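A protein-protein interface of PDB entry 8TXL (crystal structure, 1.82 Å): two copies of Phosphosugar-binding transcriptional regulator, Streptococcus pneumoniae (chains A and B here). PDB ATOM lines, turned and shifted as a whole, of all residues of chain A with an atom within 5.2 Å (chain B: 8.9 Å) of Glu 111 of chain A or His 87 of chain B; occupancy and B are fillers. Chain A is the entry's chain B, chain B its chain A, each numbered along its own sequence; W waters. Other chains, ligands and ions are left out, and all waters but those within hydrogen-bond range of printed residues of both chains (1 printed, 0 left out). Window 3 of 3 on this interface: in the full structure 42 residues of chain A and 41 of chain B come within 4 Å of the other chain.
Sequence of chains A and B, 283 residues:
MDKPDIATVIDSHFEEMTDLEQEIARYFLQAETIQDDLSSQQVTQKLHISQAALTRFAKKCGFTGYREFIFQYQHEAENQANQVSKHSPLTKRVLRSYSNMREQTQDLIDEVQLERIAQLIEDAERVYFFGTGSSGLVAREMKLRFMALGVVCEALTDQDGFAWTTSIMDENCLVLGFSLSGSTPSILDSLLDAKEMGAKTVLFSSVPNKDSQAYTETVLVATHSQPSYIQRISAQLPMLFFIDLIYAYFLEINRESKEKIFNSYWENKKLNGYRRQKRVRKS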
ATOM      1  N   GLN A 106     -30.178  -3.451 -18.242  1.00  0.00           N
ATOM      2  CA  GLN A 106     -29.444  -2.659 -17.251  1.00  0.00           C
ATOM      3  C   GLN A 106     -29.533  -3.270 -15.850  1.00  0.00           C
ATOM      4  O   GLN A 106     -28.536  -3.285 -15.120  1.00  0.00           O
ATOM      5  CB  GLN A 106     -30.022  -1.237 -17.285  1.00  0.00           C
ATOM      6  CG  GLN A 106     -29.556  -0.299 -16.249  1.00  0.00           C
ATOM      7  CD  GLN A 106     -29.893   1.139 -16.627  1.00  0.00           C
ATOM      8  OE1 GLN A 106     -30.040   1.470 -17.820  1.00  0.00           O
ATOM      9  NE2 GLN A 106     -30.062   1.983 -15.628  1.00  0.00           N
ATOM     10  N   ILE A 109     -27.163  -6.470 -15.444  1.00  0.00           N
ATOM     11  CA  ILE A 109     -25.725  -6.397 -15.612  1.00  0.00           C
ATOM     12  C   ILE A 109     -25.040  -6.797 -14.313  1.00  0.00           C
ATOM     13  O   ILE A 109     -25.297  -6.215 -13.261  1.00  0.00           O
ATOM     14  CB  ILE A 109     -25.276  -4.995 -16.058  1.00  0.00           C
ATOM     15  CG1 ILE A 109     -25.769  -4.666 -17.468  1.00  0.00           C
ATOM     16  CG2 ILE A 109     -23.733  -4.913 -16.020  1.00  0.00           C
ATOM     17  CD1 ILE A 109     -25.754  -3.176 -17.812  1.00  0.00           C
ATOM     18  N   ASP A 110     -24.129  -7.756 -14.397  1.00  0.00           N
ATOM     19  CA  ASP A 110     -23.232  -8.153 -13.320  1.00  0.00           C
ATOM     20  C   ASP A 110     -21.845  -7.711 -13.794  1.00  0.00           C
ATOM     21  O   ASP A 110     -21.166  -8.417 -14.536  1.00  0.00           O
ATOM     22  CB  ASP A 110     -23.348  -9.688 -13.063  1.00  0.00           C
ATOM     23  CG  ASP A 110     -22.381 -10.196 -12.004  1.00  0.00           C
ATOM     24  OD1 ASP A 110     -21.428  -9.488 -11.662  1.00  0.00           O
ATOM     25  OD2 ASP A 110     -22.573 -11.354 -11.555  1.00  0.00           O
ATOM     26  N   GLU A 111     -21.421  -6.518 -13.371  1.00  0.00           N
ATOM     27  CA  GLU A 111     -20.187  -5.976 -13.919  1.00  0.00           C
ATOM     28  C   GLU A 111     -18.993  -6.859 -13.585  1.00  0.00           C
ATOM     29  O   GLU A 111     -18.076  -7.001 -14.402  1.00  0.00           O
ATOM     30  CB  GLU A 111     -19.958  -4.547 -13.416  1.00  0.00           C
ATOM     31  CG  GLU A 111     -21.082  -3.595 -13.790  1.00  0.00           C
ATOM     32  CD  GLU A 111     -20.725  -2.147 -13.425  1.00  0.00           C
ATOM     33  OE1 GLU A 111     -19.964  -1.979 -12.472  1.00  0.00           O
ATOM     34  OE2 GLU A 111     -21.159  -1.219 -14.111  1.00  0.00           O
ATOM     35  N   VAL A 112     -18.955  -7.443 -12.385  1.00  0.00           N
ATOM     36  CA  VAL A 112     -17.826  -8.311 -12.074  1.00  0.00           C
ATOM     37  C   VAL A 112     -17.779  -9.495 -13.038  1.00  0.00           C
ATOM     38  O   VAL A 112     -16.712  -9.871 -13.529  1.00  0.00           O
ATOM     39  CB  VAL A 112     -17.900  -8.773 -10.621  1.00  0.00           C
ATOM     40  CG1 VAL A 112     -16.751  -9.690 -10.321  1.00  0.00           C
ATOM     41  CG2 VAL A 112     -17.794  -7.538  -9.728  1.00  0.00           C
ATOM     42  N   GLN A 113     -18.934 -10.094 -13.313  1.00  0.00           N
ATOM     43  CA  GLN A 113     -18.984 -11.220 -14.246  1.00  0.00           C
ATOM     44  C   GLN A 113     -18.465 -10.828 -15.630  1.00  0.00           C
ATOM     45  O   GLN A 113     -17.674 -11.559 -16.247  1.00  0.00           O
ATOM     46  CB  GLN A 113     -20.420 -11.736 -14.325  1.00  0.00           C
ATOM     47  CG  GLN A 113     -20.540 -12.881 -15.350  1.00  0.00           C
ATOM     48  CD  GLN A 113     -21.952 -13.370 -15.555  1.00  0.00           C
ATOM     49  OE1 GLN A 113     -22.885 -12.589 -15.783  1.00  0.00           O
ATOM     50  NE2 GLN A 113     -22.118 -14.687 -15.527  1.00  0.00           N
ATOM     51  N   LEU A 114     -18.914  -9.688 -16.152  1.00  0.00           N
ATOM     52  CA  LEU A 114     -18.562  -9.350 -17.519  1.00  0.00           C
ATOM     53  C   LEU A 114     -17.085  -9.031 -17.618  1.00  0.00           C
ATOM     54  O   LEU A 114     -16.452  -9.346 -18.624  1.00  0.00           O
ATOM     55  CB  LEU A 114     -19.418  -8.188 -18.008  1.00  0.00           C
ATOM     56  CG  LEU A 114     -20.918  -8.430 -18.003  1.00  0.00           C
ATOM     57  CD1 LEU A 114     -21.671  -7.341 -18.729  1.00  0.00           C
ATOM     58  CD2 LEU A 114     -21.250  -9.806 -18.616  1.00  0.00           C
ATOM     59  N   GLU A 115     -16.496  -8.475 -16.560  1.00  0.00           N
ATOM     60  CA  GLU A 115     -15.044  -8.318 -16.536  1.00  0.00           C
ATOM     61  C   GLU A 115     -14.377  -9.684 -16.489  1.00  0.00           C
ATOM     62  O   GLU A 115     -13.320  -9.900 -17.097  1.00  0.00           O
ATOM     63  CB  GLU A 115     -14.638  -7.432 -15.342  1.00  0.00           C
ATOM     64  CG  GLU A 115     -13.128  -7.196 -15.180  1.00  0.00           C
ATOM     65  CD  GLU A 115     -12.514  -6.377 -16.295  1.00  0.00           C
ATOM     66  OE1 GLU A 115     -13.244  -5.570 -16.893  1.00  0.00           O
ATOM     67  OE2 GLU A 115     -11.298  -6.548 -16.564  1.00  0.00           O
ATOM     68  N   ARG A 116     -15.011 -10.634 -15.818  1.00  0.00           N
ATOM     69  CA  ARG A 116     -14.413 -11.953 -15.739  1.00  0.00           C
ATOM     70  C   ARG A 116     -14.381 -12.585 -17.128  1.00  0.00           C
ATOM     71  O   ARG A 116     -13.375 -13.185 -17.533  1.00  0.00           O
ATOM     72  CB  ARG A 116     -15.188 -12.834 -14.776  1.00  0.00           C
ATOM     73  CG  ARG A 116     -14.763 -12.770 -13.312  1.00  0.00           C
ATOM     74  CD  ARG A 116     -14.985 -14.136 -12.653  1.00  0.00           C
ATOM     75  NE  ARG A 116     -16.321 -14.673 -12.882  1.00  0.00           N
ATOM     76  CZ  ARG A 116     -17.406 -14.186 -12.305  1.00  0.00           C
ATOM     77  NH1 ARG A 116     -17.326 -13.213 -11.420  1.00  0.00           N
ATOM     78  NH2 ARG A 116     -18.599 -14.679 -12.627  1.00  0.00           N
ATOM     79  N   TYR A 249     -15.491  -3.700 -22.138  1.00  0.00           N
ATOM     80  CA  TYR A 249     -14.579  -4.025 -21.052  1.00  0.00           C
ATOM     81  C   TYR A 249     -13.283  -4.585 -21.590  1.00  0.00           C
ATOM     82  O   TYR A 249     -12.200  -4.238 -21.119  1.00  0.00           O
ATOM     83  CB  TYR A 249     -15.184  -5.032 -20.069  1.00  0.00           C
ATOM     84  CG  TYR A 249     -16.409  -4.637 -19.272  1.00  0.00           C
ATOM     85  CD1 TYR A 249     -16.997  -3.398 -19.405  1.00  0.00           C
ATOM     86  CD2 TYR A 249     -16.961  -5.523 -18.354  1.00  0.00           C
ATOM     87  CE1 TYR A 249     -18.116  -3.059 -18.675  1.00  0.00           C
ATOM     88  CE2 TYR A 249     -18.071  -5.183 -17.614  1.00  0.00           C
ATOM     89  CZ  TYR A 249     -18.642  -3.949 -17.777  1.00  0.00           C
ATOM     90  OH  TYR A 249     -19.758  -3.614 -17.044  1.00  0.00           O
ATOM     91  N   VAL B  84     -29.572   5.829  -6.702  1.00  0.00           N
ATOM     92  CA  VAL B  84     -28.308   6.283  -7.243  1.00  0.00           C
ATOM     93  C   VAL B  84     -27.769   5.149  -8.105  1.00  0.00           C
ATOM     94  O   VAL B  84     -27.885   3.981  -7.732  1.00  0.00           O
ATOM     95  CB  VAL B  84     -27.320   6.650  -6.128  1.00  0.00           C
ATOM     96  CG1 VAL B  84     -25.976   6.975  -6.754  1.00  0.00           C
ATOM     97  CG2 VAL B  84     -27.857   7.830  -5.307  1.00  0.00           C
ATOM     98  N   SER B  85     -27.203   5.470  -9.257  1.00  0.00           N
ATOM     99  CA  SER B  85     -26.725   4.397 -10.115  1.00  0.00           C
ATOM    100  C   SER B  85     -25.577   3.641  -9.466  1.00  0.00           C
ATOM    101  O   SER B  85     -24.653   4.235  -8.912  1.00  0.00           O
ATOM    102  CB  SER B  85     -26.244   4.920 -11.479  1.00  0.00           C
ATOM    103  OG  SER B  85     -25.662   3.818 -12.193  1.00  0.00           O
ATOM    104  N   LYS B  86     -25.572   2.324  -9.665  1.00  0.00           N
ATOM    105  CA  LYS B  86     -24.486   1.474  -9.202  1.00  0.00           C
ATOM    106  C   LYS B  86     -23.492   1.078 -10.303  1.00  0.00           C
ATOM    107  O   LYS B  86     -22.586   0.284 -10.039  1.00  0.00           O
ATOM    108  CB  LYS B  86     -25.068   0.210  -8.563  1.00  0.00           C
ATOM    109  CG  LYS B  86     -26.093  -0.547  -9.426  1.00  0.00           C
ATOM    110  CD  LYS B  86     -26.829  -1.631  -8.627  1.00  0.00           C
ATOM    111  CE  LYS B  86     -26.229  -3.013  -8.862  1.00  0.00           C
ATOM    112  NZ  LYS B  86     -26.540  -3.511 -10.239  1.00  0.00           N
ATOM    113  N   HIS B  87     -23.599   1.635 -11.500  1.00  0.00           N
ATOM    114  CA  HIS B  87     -22.761   1.190 -12.605  1.00  0.00           C
ATOM    115  C   HIS B  87     -21.530   2.052 -12.810  1.00  0.00           C
ATOM    116  O   HIS B  87     -21.469   3.212 -12.405  1.00  0.00           O
ATOM    117  CB  HIS B  87     -23.595   1.146 -13.883  1.00  0.00           C
ATOM    118  CG  HIS B  87     -24.688   0.138 -13.817  1.00  0.00           C
ATOM    119  ND1 HIS B  87     -25.980   0.408 -14.217  1.00  0.00           N
ATOM    120  CD2 HIS B  87     -24.688  -1.134 -13.339  1.00  0.00           C
ATOM    121  CE1 HIS B  87     -26.726  -0.662 -13.993  1.00  0.00           C
ATOM    122  NE2 HIS B  87     -25.966  -1.609 -13.463  1.00  0.00           N
ATOM    123  N   SER B  88     -20.548   1.440 -13.455  1.00  0.00           N
ATOM    124  CA  SER B  88     -19.280   2.030 -13.796  1.00  0.00           C
ATOM    125  C   SER B  88     -19.416   2.943 -15.011  1.00  0.00           C
ATOM    126  O   SER B  88     -20.390   2.863 -15.770  1.00  0.00           O
ATOM    127  CB  SER B  88     -18.265   0.931 -14.079  1.00  0.00           C
ATOM    128  OG  SER B  88     -18.403   0.448 -15.424  1.00  0.00           O
ATOM    129  N   PRO B  89     -18.497   3.889 -15.158  1.00  0.00           N
ATOM    130  CA  PRO B  89     -18.564   4.773 -16.325  1.00  0.00           C
ATOM    131  C   PRO B  89     -18.636   4.008 -17.623  1.00  0.00           C
ATOM    132  O   PRO B  89     -19.335   4.418 -18.564  1.00  0.00           O
ATOM    133  CB  PRO B  89     -17.261   5.578 -16.232  1.00  0.00           C
ATOM    134  CG  PRO B  89     -16.949   5.620 -14.739  1.00  0.00           C
ATOM    135  CD  PRO B  89     -17.564   4.380 -14.122  1.00  0.00           C
ATOM    136  N   LEU B  90     -17.807   2.975 -17.722  1.00  0.00           N
ATOM    137  CA  LEU B  90     -17.765   2.166 -18.935  1.00  0.00           C
ATOM    138  C   LEU B  90     -19.151   1.624 -19.280  1.00  0.00           C
ATOM    139  O   LEU B  90     -19.640   1.779 -20.416  1.00  0.00           O
ATOM    140  CB  LEU B  90     -16.780   1.004 -18.745  1.00  0.00           C
ATOM    141  CG  LEU B  90     -15.612   0.882 -19.718  1.00  0.00           C
ATOM    142  CD1 LEU B  90     -14.825  -0.427 -19.577  1.00  0.00           C
ATOM    143  CD2 LEU B  90     -16.082   1.089 -21.163  1.00  0.00           C
ATOM    144  N   THR B  91     -19.792   0.972 -18.308  1.00  0.00           N
ATOM    145  CA  THR B  91     -21.160   0.485 -18.470  1.00  0.00           C
ATOM    146  C   THR B  91     -22.115   1.581 -18.906  1.00  0.00           C
ATOM    147  O   THR B  91     -22.985   1.359 -19.760  1.00  0.00           O
ATOM    148  CB  THR B  91     -21.645  -0.114 -17.153  1.00  0.00           C
ATOM    149  OG1 THR B  91     -20.762  -1.167 -16.810  1.00  0.00           O
ATOM    150  CG2 THR B  91     -23.040  -0.602 -17.249  1.00  0.00           C
ATOM    151  N   LYS B  92     -22.042   2.751 -18.274  1.00  0.00           N
ATOM    152  CA  LYS B  92     -22.987   3.795 -18.625  1.00  0.00           C
ATOM    153  C   LYS B  92     -22.761   4.259 -20.057  1.00  0.00           C
ATOM    154  O   LYS B  92     -23.721   4.570 -20.764  1.00  0.00           O
ATOM    155  CB  LYS B  92     -22.865   4.964 -17.640  1.00  0.00           C
ATOM    156  CG  LYS B  92     -23.250   4.602 -16.195  1.00  0.00           C
ATOM    157  CD  LYS B  92     -23.083   5.845 -15.319  1.00  0.00           C
ATOM    158  CE  LYS B  92     -22.969   5.529 -13.863  1.00  0.00           C
ATOM    159  NZ  LYS B  92     -22.637   6.795 -13.122  1.00  0.00           N
ATOM    160  N   ARG B  93     -21.496   4.327 -20.485  1.00  0.00           N
ATOM    161  CA  ARG B  93     -21.197   4.722 -21.860  1.00  0.00           C
ATOM    162  C   ARG B  93     -21.900   3.802 -22.856  1.00  0.00           C
ATOM    163  O   ARG B  93     -22.505   4.267 -23.829  1.00  0.00           O
ATOM    164  CB  ARG B  93     -19.696   4.678 -22.107  1.00  0.00           C
ATOM    165  CG  ARG B  93     -19.249   5.332 -23.433  1.00  0.00           C
ATOM    166  CD  ARG B  93     -17.799   4.962 -23.777  1.00  0.00           C
ATOM    167  NE  ARG B  93     -17.746   3.630 -24.383  1.00  0.00           N
ATOM    168  CZ  ARG B  93     -16.679   2.841 -24.422  1.00  0.00           C
ATOM    169  NH1 ARG B  93     -15.532   3.192 -23.860  1.00  0.00           N
ATOM    170  NH2 ARG B  93     -16.766   1.661 -25.037  1.00  0.00           N
ATOM    171  N   LEU B  95     -24.578   1.761 -22.371  1.00  0.00           N
ATOM    172  CA  LEU B  95     -26.007   1.995 -22.251  1.00  0.00           C
ATOM    173  C   LEU B  95     -26.419   3.313 -22.912  1.00  0.00           C
ATOM    174  O   LEU B  95     -27.467   3.404 -23.570  1.00  0.00           O
ATOM    175  CB  LEU B  95     -26.386   2.032 -20.761  1.00  0.00           C
ATOM    176  CG  LEU B  95     -26.254   0.721 -19.942  1.00  0.00           C
ATOM    177  CD1 LEU B  95     -26.476   0.885 -18.432  1.00  0.00           C
ATOM    178  CD2 LEU B  95     -27.327  -0.225 -20.485  1.00  0.00           C
HETATM  179  O   HOH W   1     -26.966  -4.228 -12.617  1.00  0.00           O
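NE2 of His 87 of chain B sits close to O of Gln 106 of chain A. The side-chain carboxylate of Glu 111 of chain A sits at hydrogen-bond distance from the backbone NH of Ser 88 of chain B (2.8 Å). OG1 of Thr 91 of chain B is in hydrogen-bond range of OE2 of Glu 111 of chain A. The side-chain hydroxyl (OG1) of Thr 91 of chain B sits at hydrogen-bond distance from the side-chain hydroxyl (OH) of Tyr 249 of chain A, at 2.7 Å.
CD1 of Leu 95 of chain B touches OE1 of Gln 106 of chain A (3.7 Å). Thr 91 of chain B touches Ile 109 of chain A (CG2 to CD1, 3.8 Å). Glu 111 of chain A touches His 87 of chain B. CD1 of Tyr 249 of chain A touches CD1 of Leu 90 of chain B, 3.7 Å away.
Water W1 lies within hydrogen-bond range of the side-chain amino group of Lys 86 of chain B (2.5 Å), the backbone carbonyl oxygen of Ile 109 of chain A (2.7 Å), a ring nitrogen (NE2) of His 87 of chain B (2.9 Å) and the backbone carbonyl oxygen of Gln 106 of chain A (3.1 Å).
Glu 111 of chain A touches just these residues of chain B: His 87 (3.3 Å), Ser 88 (2.8 Å) and Thr 91 (2.7 Å). Of the printed residues of chain A, Leu 95 of chain B touches Gln 106 (3.7 Å). Of the printed residues of chain B, Ile 109 of chain A touches Thr 91 (3.8 Å). Printed residues of chain B within 4 Å of Tyr 249 of chain A: Leu 90 (3.7 Å) and Thr 91 (2.7 Å). Printed residues of chain A within 4 Å of Ser 88 of chain B: Glu 111. Printed residues of chain B within 4 Å of Gln 106 of chain A: His 87 (3.4 Å) and Leu 95 (3.7 Å). Lys 92 of chain B touches none of the printed residues of chain A. Lys 86 of chain B touches none of the printed residues of chain A. The nearest residue of chain B that does not touch Glu 111 of chain A is Lys 86 of chain B (4.2 Å). The nearest printed residue of chain A that does not touch Leu 95 of chain B is Ile 109 of chain A (4.2 Å).
No position is printed for both chains. Of the 8 pairs that touch across the chains among the printed residues, none has its exchanged pair printed and touching as well.
The backbone NH (N) of His 87 of chain B lies within hydrogen-bond range of the side-chain hydroxyl (OG) of Ser 85 of chain B, at 3.1 Å. OG of Ser 88 of chain B sits close to N of Leu 90 of chain B, at 3.5 Å. OG of Ser 88 of chain B lies within hydrogen-bond range of OG1 of Thr 91 of chain B (3.2 Å).
Printed residues of chain B that touch a printed residue of chain A: His 87, Ser 88, Leu 90, Thr 91 and Leu 95. Hydrophobic or aromatic side chains of chain B within 4 Å of the printed part of chain A: His 87, Leu 90 and Leu 95. Along chain B the printed residues that touch a printed residue of chain A span positions 87 to 95. Of the 10 printed residues of chain A, 4 touch a printed residue of chain B. Among the printed residues, no Asp or Glu carboxylate lies within 4 Å of a Lys or Arg side-chain nitrogen of the other chain.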
